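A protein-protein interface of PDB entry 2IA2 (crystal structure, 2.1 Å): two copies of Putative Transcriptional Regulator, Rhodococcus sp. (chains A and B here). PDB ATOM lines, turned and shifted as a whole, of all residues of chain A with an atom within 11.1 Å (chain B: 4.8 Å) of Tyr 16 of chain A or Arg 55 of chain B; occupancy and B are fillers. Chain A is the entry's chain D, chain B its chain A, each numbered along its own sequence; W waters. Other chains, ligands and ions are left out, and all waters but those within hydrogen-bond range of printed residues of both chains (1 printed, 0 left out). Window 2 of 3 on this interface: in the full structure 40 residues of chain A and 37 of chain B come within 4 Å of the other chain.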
ATOM      1  N   TYR A  16      -7.171  34.487 -29.347  1.00  0.00           N
ATOM      2  CA  TYR A  16      -8.392  33.606 -29.299  1.00  0.00           C
ATOM      3  C   TYR A  16      -8.050  32.204 -29.796  1.00  0.00           C
ATOM      4  O   TYR A  16      -7.538  32.032 -30.907  1.00  0.00           O
ATOM      5  CB  TYR A  16      -9.569  34.191 -30.108  1.00  0.00           C
ATOM      6  CG  TYR A  16     -10.880  33.356 -30.107  1.00  0.00           C
ATOM      7  CD1 TYR A  16     -11.882  33.587 -29.154  1.00  0.00           C
ATOM      8  CD2 TYR A  16     -11.115  32.362 -31.063  1.00  0.00           C
ATOM      9  CE1 TYR A  16     -13.074  32.859 -29.143  1.00  0.00           C
ATOM     10  CE2 TYR A  16     -12.326  31.627 -31.074  1.00  0.00           C
ATOM     11  CZ  TYR A  16     -13.292  31.888 -30.099  1.00  0.00           C
ATOM     12  OH  TYR A  16     -14.484  31.190 -30.082  1.00  0.00           O
ATOM     13  N   VAL A  17      -8.358  31.213 -28.964  1.00  0.00           N
ATOM     14  CA  VAL A  17      -8.037  29.823 -29.218  1.00  0.00           C
ATOM     15  C   VAL A  17      -9.304  29.060 -29.647  1.00  0.00           C
ATOM     16  O   VAL A  17     -10.096  28.634 -28.818  1.00  0.00           O
ATOM     17  CB  VAL A  17      -7.426  29.205 -27.943  1.00  0.00           C
ATOM     18  CG1 VAL A  17      -7.015  27.728 -28.186  1.00  0.00           C
ATOM     19  CG2 VAL A  17      -6.248  30.091 -27.432  1.00  0.00           C
ATOM     20  N   GLN A  18      -9.469  28.865 -30.959  1.00  0.00           N
ATOM     21  CA  GLN A  18     -10.669  28.252 -31.495  1.00  0.00           C
ATOM     22  C   GLN A  18     -10.866  26.805 -31.075  1.00  0.00           C
ATOM     23  O   GLN A  18     -11.996  26.359 -30.873  1.00  0.00           O
ATOM     24  CB  GLN A  18     -10.694  28.382 -33.023  1.00  0.00           C
ATOM     25  CG  GLN A  18     -11.934  27.793 -33.666  1.00  0.00           C
ATOM     26  CD  GLN A  18     -11.819  27.759 -35.170  1.00  0.00           C
ATOM     27  OE1 GLN A  18     -11.796  26.682 -35.783  1.00  0.00           O
ATOM     28  NE2 GLN A  18     -11.768  28.939 -35.786  1.00  0.00           N
ATOM     29  N   SER A  19      -9.799  26.041 -30.940  1.00  0.00           N
ATOM     30  CA  SER A  19     -10.001  24.652 -30.564  1.00  0.00           C
ATOM     31  C   SER A  19     -10.503  24.526 -29.124  1.00  0.00           C
ATOM     32  O   SER A  19     -11.236  23.579 -28.799  1.00  0.00           O
ATOM     33  CB  SER A  19      -8.758  23.798 -30.833  1.00  0.00           C
ATOM     34  OG  SER A  19      -7.637  24.387 -30.194  1.00  0.00           O
ATOM     35  N   LEU A  20     -10.121  25.473 -28.269  1.00  0.00           N
ATOM     36  CA  LEU A  20     -10.733  25.617 -26.945  1.00  0.00           C
ATOM     37  C   LEU A  20     -12.257  25.845 -27.016  1.00  0.00           C
ATOM     38  O   LEU A  20     -13.038  25.124 -26.361  1.00  0.00           O
ATOM     39  CB  LEU A  20     -10.058  26.748 -26.111  1.00  0.00           C
ATOM     40  CG  LEU A  20     -10.613  26.998 -24.692  1.00  0.00           C
ATOM     41  CD1 LEU A  20     -10.638  25.710 -23.919  1.00  0.00           C
ATOM     42  CD2 LEU A  20      -9.810  28.074 -23.961  1.00  0.00           C
ATOM     43  N   ALA A  21     -12.672  26.831 -27.801  1.00  0.00           N
ATOM     44  CA  ALA A  21     -14.087  27.139 -27.991  1.00  0.00           C
ATOM     45  C   ALA A  21     -14.897  25.909 -28.421  1.00  0.00           C
ATOM     46  O   ALA A  21     -15.987  25.630 -27.882  1.00  0.00           O
ATOM     47  CB  ALA A  21     -14.251  28.287 -28.985  1.00  0.00           C
ATOM     48  N   ARG A  22     -14.345  25.163 -29.366  1.00  0.00           N
ATOM     49  CA  ARG A  22     -15.012  23.993 -29.921  1.00  0.00           C
ATOM     50  C   ARG A  22     -15.081  22.823 -28.915  1.00  0.00           C
ATOM     51  O   ARG A  22     -16.135  22.202 -28.760  1.00  0.00           O
ATOM     52  CB  ARG A  22     -14.358  23.589 -31.232  1.00  0.00           C
ATOM     53  CG  ARG A  22     -14.358  24.705 -32.278  1.00  0.00           C
ATOM     54  CD  ARG A  22     -13.694  24.276 -33.593  1.00  0.00           C
ATOM     55  NE  ARG A  22     -14.180  25.048 -34.735  1.00  0.00           N
ATOM     56  CZ  ARG A  22     -13.982  24.711 -36.007  1.00  0.00           C
ATOM     57  NH1 ARG A  22     -13.291  23.614 -36.312  1.00  0.00           N
ATOM     58  NH2 ARG A  22     -14.470  25.468 -36.990  1.00  0.00           N
ATOM     59  N   GLY A  23     -13.967  22.560 -28.225  1.00  0.00           N
ATOM     60  CA  GLY A  23     -13.927  21.543 -27.186  1.00  0.00           C
ATOM     61  C   GLY A  23     -14.976  21.817 -26.108  1.00  0.00           C
ATOM     62  O   GLY A  23     -15.640  20.896 -25.624  1.00  0.00           O
ATOM     63  N   LEU A  24     -15.190  23.080 -25.773  1.00  0.00           N
ATOM     64  CA  LEU A  24     -16.181  23.390 -24.756  1.00  0.00           C
ATOM     65  C   LEU A  24     -17.599  23.290 -25.312  1.00  0.00           C
ATOM     66  O   LEU A  24     -18.522  22.896 -24.585  1.00  0.00           O
ATOM     67  CB  LEU A  24     -15.927  24.761 -24.118  1.00  0.00           C
ATOM     68  CG  LEU A  24     -14.714  24.879 -23.187  1.00  0.00           C
ATOM     69  CD1 LEU A  24     -14.261  26.333 -22.998  1.00  0.00           C
ATOM     70  CD2 LEU A  24     -14.979  24.167 -21.790  1.00  0.00           C
ATOM     71  N   ALA A  25     -17.781  23.642 -26.587  1.00  0.00           N
ATOM     72  CA  ALA A  25     -19.063  23.478 -27.235  1.00  0.00           C
ATOM     73  C   ALA A  25     -19.437  21.992 -27.274  1.00  0.00           C
ATOM     74  O   ALA A  25     -20.609  21.645 -27.162  1.00  0.00           O
ATOM     75  CB  ALA A  25     -19.049  24.066 -28.661  1.00  0.00           C
ATOM     76  N   THR A  46     -22.720  20.131 -32.900  1.00  0.00           N
ATOM     77  CA  THR A  46     -21.843  21.291 -32.728  1.00  0.00           C
ATOM     78  C   THR A  46     -21.392  21.938 -34.050  1.00  0.00           C
ATOM     79  O   THR A  46     -20.558  22.857 -34.043  1.00  0.00           O
ATOM     80  CB  THR A  46     -20.599  20.894 -31.919  1.00  0.00           C
ATOM     81  N   PHE A  56     -11.547  16.139 -30.545  1.00  0.00           N
ATOM     82  CA  PHE A  56     -12.112  16.592 -29.299  1.00  0.00           C
ATOM     83  C   PHE A  56     -12.574  15.480 -28.359  1.00  0.00           C
ATOM     84  O   PHE A  56     -12.087  15.374 -27.258  1.00  0.00           O
ATOM     85  CB  PHE A  56     -13.196  17.600 -29.569  1.00  0.00           C
ATOM     86  CG  PHE A  56     -12.701  18.857 -30.185  1.00  0.00           C
ATOM     87  CD1 PHE A  56     -11.622  19.516 -29.667  1.00  0.00           C
ATOM     88  CD2 PHE A  56     -13.313  19.382 -31.281  1.00  0.00           C
ATOM     89  CE1 PHE A  56     -11.175  20.659 -30.213  1.00  0.00           C
ATOM     90  CE2 PHE A  56     -12.851  20.519 -31.848  1.00  0.00           C
ATOM     91  CZ  PHE A  56     -11.772  21.159 -31.307  1.00  0.00           C
ATOM     92  N   ALA B  51       2.510  34.202 -21.441  1.00  0.00           N
ATOM     93  CA  ALA B  51       2.014  34.335 -22.839  1.00  0.00           C
ATOM     94  C   ALA B  51       1.040  33.214 -23.239  1.00  0.00           C
ATOM     95  O   ALA B  51      -0.003  33.491 -23.887  1.00  0.00           O
ATOM     96  CB  ALA B  51       3.173  34.444 -23.848  1.00  0.00           C
ATOM     97  N   THR B  52       1.345  31.964 -22.860  1.00  0.00           N
ATOM     98  CA  THR B  52       0.427  30.872 -23.179  1.00  0.00           C
ATOM     99  C   THR B  52      -0.828  30.935 -22.301  1.00  0.00           C
ATOM    100  O   THR B  52      -1.922  30.831 -22.832  1.00  0.00           O
ATOM    101  CB  THR B  52       1.063  29.469 -23.129  1.00  0.00           C
ATOM    102  OG1 THR B  52       1.702  29.312 -21.875  1.00  0.00           O
ATOM    103  CG2 THR B  52       2.148  29.308 -24.246  1.00  0.00           C
ATOM    104  N   ALA B  53      -0.673  31.119 -20.990  1.00  0.00           N
ATOM    105  CA  ALA B  53      -1.838  31.298 -20.103  1.00  0.00           C
ATOM    106  C   ALA B  53      -2.785  32.424 -20.550  1.00  0.00           C
ATOM    107  O   ALA B  53      -4.011  32.264 -20.485  1.00  0.00           O
ATOM    108  CB  ALA B  53      -1.370  31.537 -18.620  1.00  0.00           C
ATOM    109  N   ARG B  54      -2.214  33.571 -20.957  1.00  0.00           N
ATOM    110  CA  ARG B  54      -2.986  34.729 -21.387  1.00  0.00           C
ATOM    111  C   ARG B  54      -3.953  34.375 -22.520  1.00  0.00           C
ATOM    112  O   ARG B  54      -5.139  34.757 -22.474  1.00  0.00           O
ATOM    113  CB  ARG B  54      -2.088  35.891 -21.797  1.00  0.00           C
ATOM    114  CG  ARG B  54      -2.865  37.114 -22.303  1.00  0.00           C
ATOM    115  CD  ARG B  54      -1.946  38.256 -22.808  1.00  0.00           C
ATOM    116  NE  ARG B  54      -1.072  38.773 -21.751  1.00  0.00           N
ATOM    117  CZ  ARG B  54       0.250  38.577 -21.654  1.00  0.00           C
ATOM    118  NH1 ARG B  54       0.950  37.873 -22.550  1.00  0.00           N
ATOM    119  NH2 ARG B  54       0.883  39.102 -20.626  1.00  0.00           N
ATOM    120  N   ARG B  55      -3.446  33.638 -23.516  1.00  0.00           N
ATOM    121  CA  ARG B  55      -4.247  33.218 -24.669  1.00  0.00           C
ATOM    122  C   ARG B  55      -5.476  32.446 -24.203  1.00  0.00           C
ATOM    123  O   ARG B  55      -6.567  32.703 -24.679  1.00  0.00           O
ATOM    124  CB  ARG B  55      -3.439  32.366 -25.657  1.00  0.00           C
ATOM    125  CG  ARG B  55      -2.439  33.167 -26.499  1.00  0.00           C
ATOM    126  CD  ARG B  55      -1.848  32.333 -27.718  1.00  0.00           C
ATOM    127  NE  ARG B  55      -2.812  32.080 -28.818  1.00  0.00           N
ATOM    128  CZ  ARG B  55      -3.282  30.877 -29.186  1.00  0.00           C
ATOM    129  NH1 ARG B  55      -2.908  29.752 -28.555  1.00  0.00           N
ATOM    130  NH2 ARG B  55      -4.137  30.803 -30.202  1.00  0.00           N
ATOM    131  N   PHE B  56      -5.298  31.512 -23.278  1.00  0.00           N
ATOM    132  CA  PHE B  56      -6.417  30.731 -22.804  1.00  0.00           C
ATOM    133  C   PHE B  56      -7.392  31.571 -21.967  1.00  0.00           C
ATOM    134  O   PHE B  56      -8.610  31.516 -22.183  1.00  0.00           O
ATOM    135  CB  PHE B  56      -5.935  29.478 -22.047  1.00  0.00           C
ATOM    136  CG  PHE B  56      -5.097  28.596 -22.893  1.00  0.00           C
ATOM    137  CD1 PHE B  56      -3.720  28.557 -22.724  1.00  0.00           C
ATOM    138  CD2 PHE B  56      -5.671  27.869 -23.936  1.00  0.00           C
ATOM    139  CE1 PHE B  56      -2.930  27.786 -23.560  1.00  0.00           C
ATOM    140  CE2 PHE B  56      -4.882  27.093 -24.772  1.00  0.00           C
ATOM    141  CZ  PHE B  56      -3.507  27.067 -24.595  1.00  0.00           C
ATOM    142  N   LEU B  57      -6.847  32.335 -21.027  1.00  0.00           N
ATOM    143  CA  LEU B  57      -7.641  33.235 -20.222  1.00  0.00           C
ATOM    144  C   LEU B  57      -8.436  34.191 -21.102  1.00  0.00           C
ATOM    145  O   LEU B  57      -9.608  34.431 -20.841  1.00  0.00           O
ATOM    146  CB  LEU B  57      -6.779  34.026 -19.259  1.00  0.00           C
ATOM    147  CG  LEU B  57      -6.335  33.235 -18.039  1.00  0.00           C
ATOM    148  CD1 LEU B  57      -5.211  34.011 -17.334  1.00  0.00           C
ATOM    149  CD2 LEU B  57      -7.554  32.913 -17.084  1.00  0.00           C
ATOM    150  N   LEU B  58      -7.832  34.740 -22.148  1.00  0.00           N
ATOM    151  CA  LEU B  58      -8.591  35.722 -22.952  1.00  0.00           C
ATOM    152  C   LEU B  58      -9.672  35.058 -23.783  1.00  0.00           C
ATOM    153  O   LEU B  58     -10.710  35.647 -24.055  1.00  0.00           O
ATOM    154  CB  LEU B  58      -7.682  36.599 -23.818  1.00  0.00           C
ATOM    155  CG  LEU B  58      -6.734  37.548 -23.061  1.00  0.00           C
ATOM    156  CD1 LEU B  58      -5.832  38.364 -24.032  1.00  0.00           C
ATOM    157  CD2 LEU B  58      -7.524  38.460 -22.116  1.00  0.00           C
ATOM    158  N   THR B  59      -9.461  33.804 -24.142  1.00  0.00           N
ATOM    159  CA  THR B  59     -10.497  33.083 -24.865  1.00  0.00           C
ATOM    160  C   THR B  59     -11.620  32.814 -23.922  1.00  0.00           C
ATOM    161  O   THR B  59     -12.759  33.083 -24.244  1.00  0.00           O
ATOM    162  CB  THR B  59      -9.948  31.802 -25.507  1.00  0.00           C
ATOM    163  OG1 THR B  59      -8.904  32.191 -26.400  1.00  0.00           O
ATOM    164  CG2 THR B  59     -11.016  31.069 -26.311  1.00  0.00           C
ATOM    165  N   GLU B  62     -13.657  35.919 -23.431  1.00  0.00           N
ATOM    166  CA  GLU B  62     -14.478  36.086 -24.619  1.00  0.00           C
ATOM    167  C   GLU B  62     -15.701  35.149 -24.608  1.00  0.00           C
ATOM    168  O   GLU B  62     -16.822  35.568 -24.928  1.00  0.00           O
ATOM    169  CB  GLU B  62     -13.612  35.883 -25.887  1.00  0.00           C
ATOM    170  CG  GLU B  62     -14.224  36.416 -27.162  1.00  0.00           C
ATOM    171  CD  GLU B  62     -13.174  36.974 -28.181  1.00  0.00           C
ATOM    172  OE1 GLU B  62     -11.908  36.853 -27.991  1.00  0.00           O
ATOM    173  OE2 GLU B  62     -13.637  37.542 -29.210  1.00  0.00           O
ATOM    174  N   LEU B  63     -15.486  33.886 -24.227  1.00  0.00           N
ATOM    175  CA  LEU B  63     -16.543  32.896 -24.137  1.00  0.00           C
ATOM    176  C   LEU B  63     -17.479  33.103 -22.951  1.00  0.00           C
ATOM    177  O   LEU B  63     -18.540  32.497 -22.905  1.00  0.00           O
ATOM    178  CB  LEU B  63     -15.946  31.493 -24.101  1.00  0.00           C
ATOM    179  CG  LEU B  63     -15.283  31.077 -25.414  1.00  0.00           C
ATOM    180  CD1 LEU B  63     -14.602  29.763 -25.288  1.00  0.00           C
ATOM    181  CD2 LEU B  63     -16.356  30.988 -26.536  1.00  0.00           C
HETATM  182  O   HOH W   1      -4.406  33.495 -31.429  1.00  0.00           O
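OG1 of Thr 59 of chain B is in hydrogen-bond range of N of Val 17 of chain A.
The side-chain hydroxyl of Thr 59 of chain B is in hydrogen-bond range of the backbone carbonyl oxygen of Arg 55 of chain B (2.9 Å).
NH2 of Arg 55 of chain B touches O of Tyr 16 of chain A (3.7 Å). OG1 of Thr 59 of chain B touches CA of Tyr 16 of chain A, at 3.3 Å. CD1 of Tyr 16 of chain A touches OE1 of Glu 62 of chain B (3.5 Å). Val 17 of chain A touches Arg 55 of chain B (CG2 to CZ, 3.5 Å). Leu 20 of chain A touches Thr 59 of chain B (CD2 to CG2, 3.99 Å). Ala 21 of chain A touches Leu 63 of chain B (CA to CD1, 3.8 Å).
Printed residues of chain B within 4 Å of Tyr 16 of chain A: Arg 55 (3.7 Å), Thr 59 (3.3 Å) and Glu 62 (3.5 Å). No residue of chain A comes within 4 Å of Ala 51 of chain B. No residue of chain A comes within 4 Å of Ala 53 of chain B. No residue of chain A comes within 4 Å of Leu 58 of chain B. Glu 62 of chain B touches just one residue of chain A: Tyr 16. Of the printed residues of chain A, Leu 63 of chain B touches Ala 21. Printed residues of chain B within 4 Å of Leu 20 of chain A: Thr 59. Gln 18 of chain A touches none of the printed residues of chain B. Leu 24 of chain A touches none of the printed residues of chain B. The nearest printed residue of chain A that does not touch Arg 55 of chain B is Leu 20 of chain A (5.7 Å).
Printed residues of chain A that touch a printed residue of chain B: Tyr 16, Val 17, Leu 20 and Ala 21. Hydrophobic or aromatic side chains of chain A that line the printed part of chain B: Tyr 16, Val 17, Leu 20 and Ala 21. Along chain A the printed residues that touch a printed residue of chain B span positions 16 to 21.
Position printed for both chains: 56.
Water W1 bridges NH2 of Arg 55 of chain B and O of Tyr 16 of chain A.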
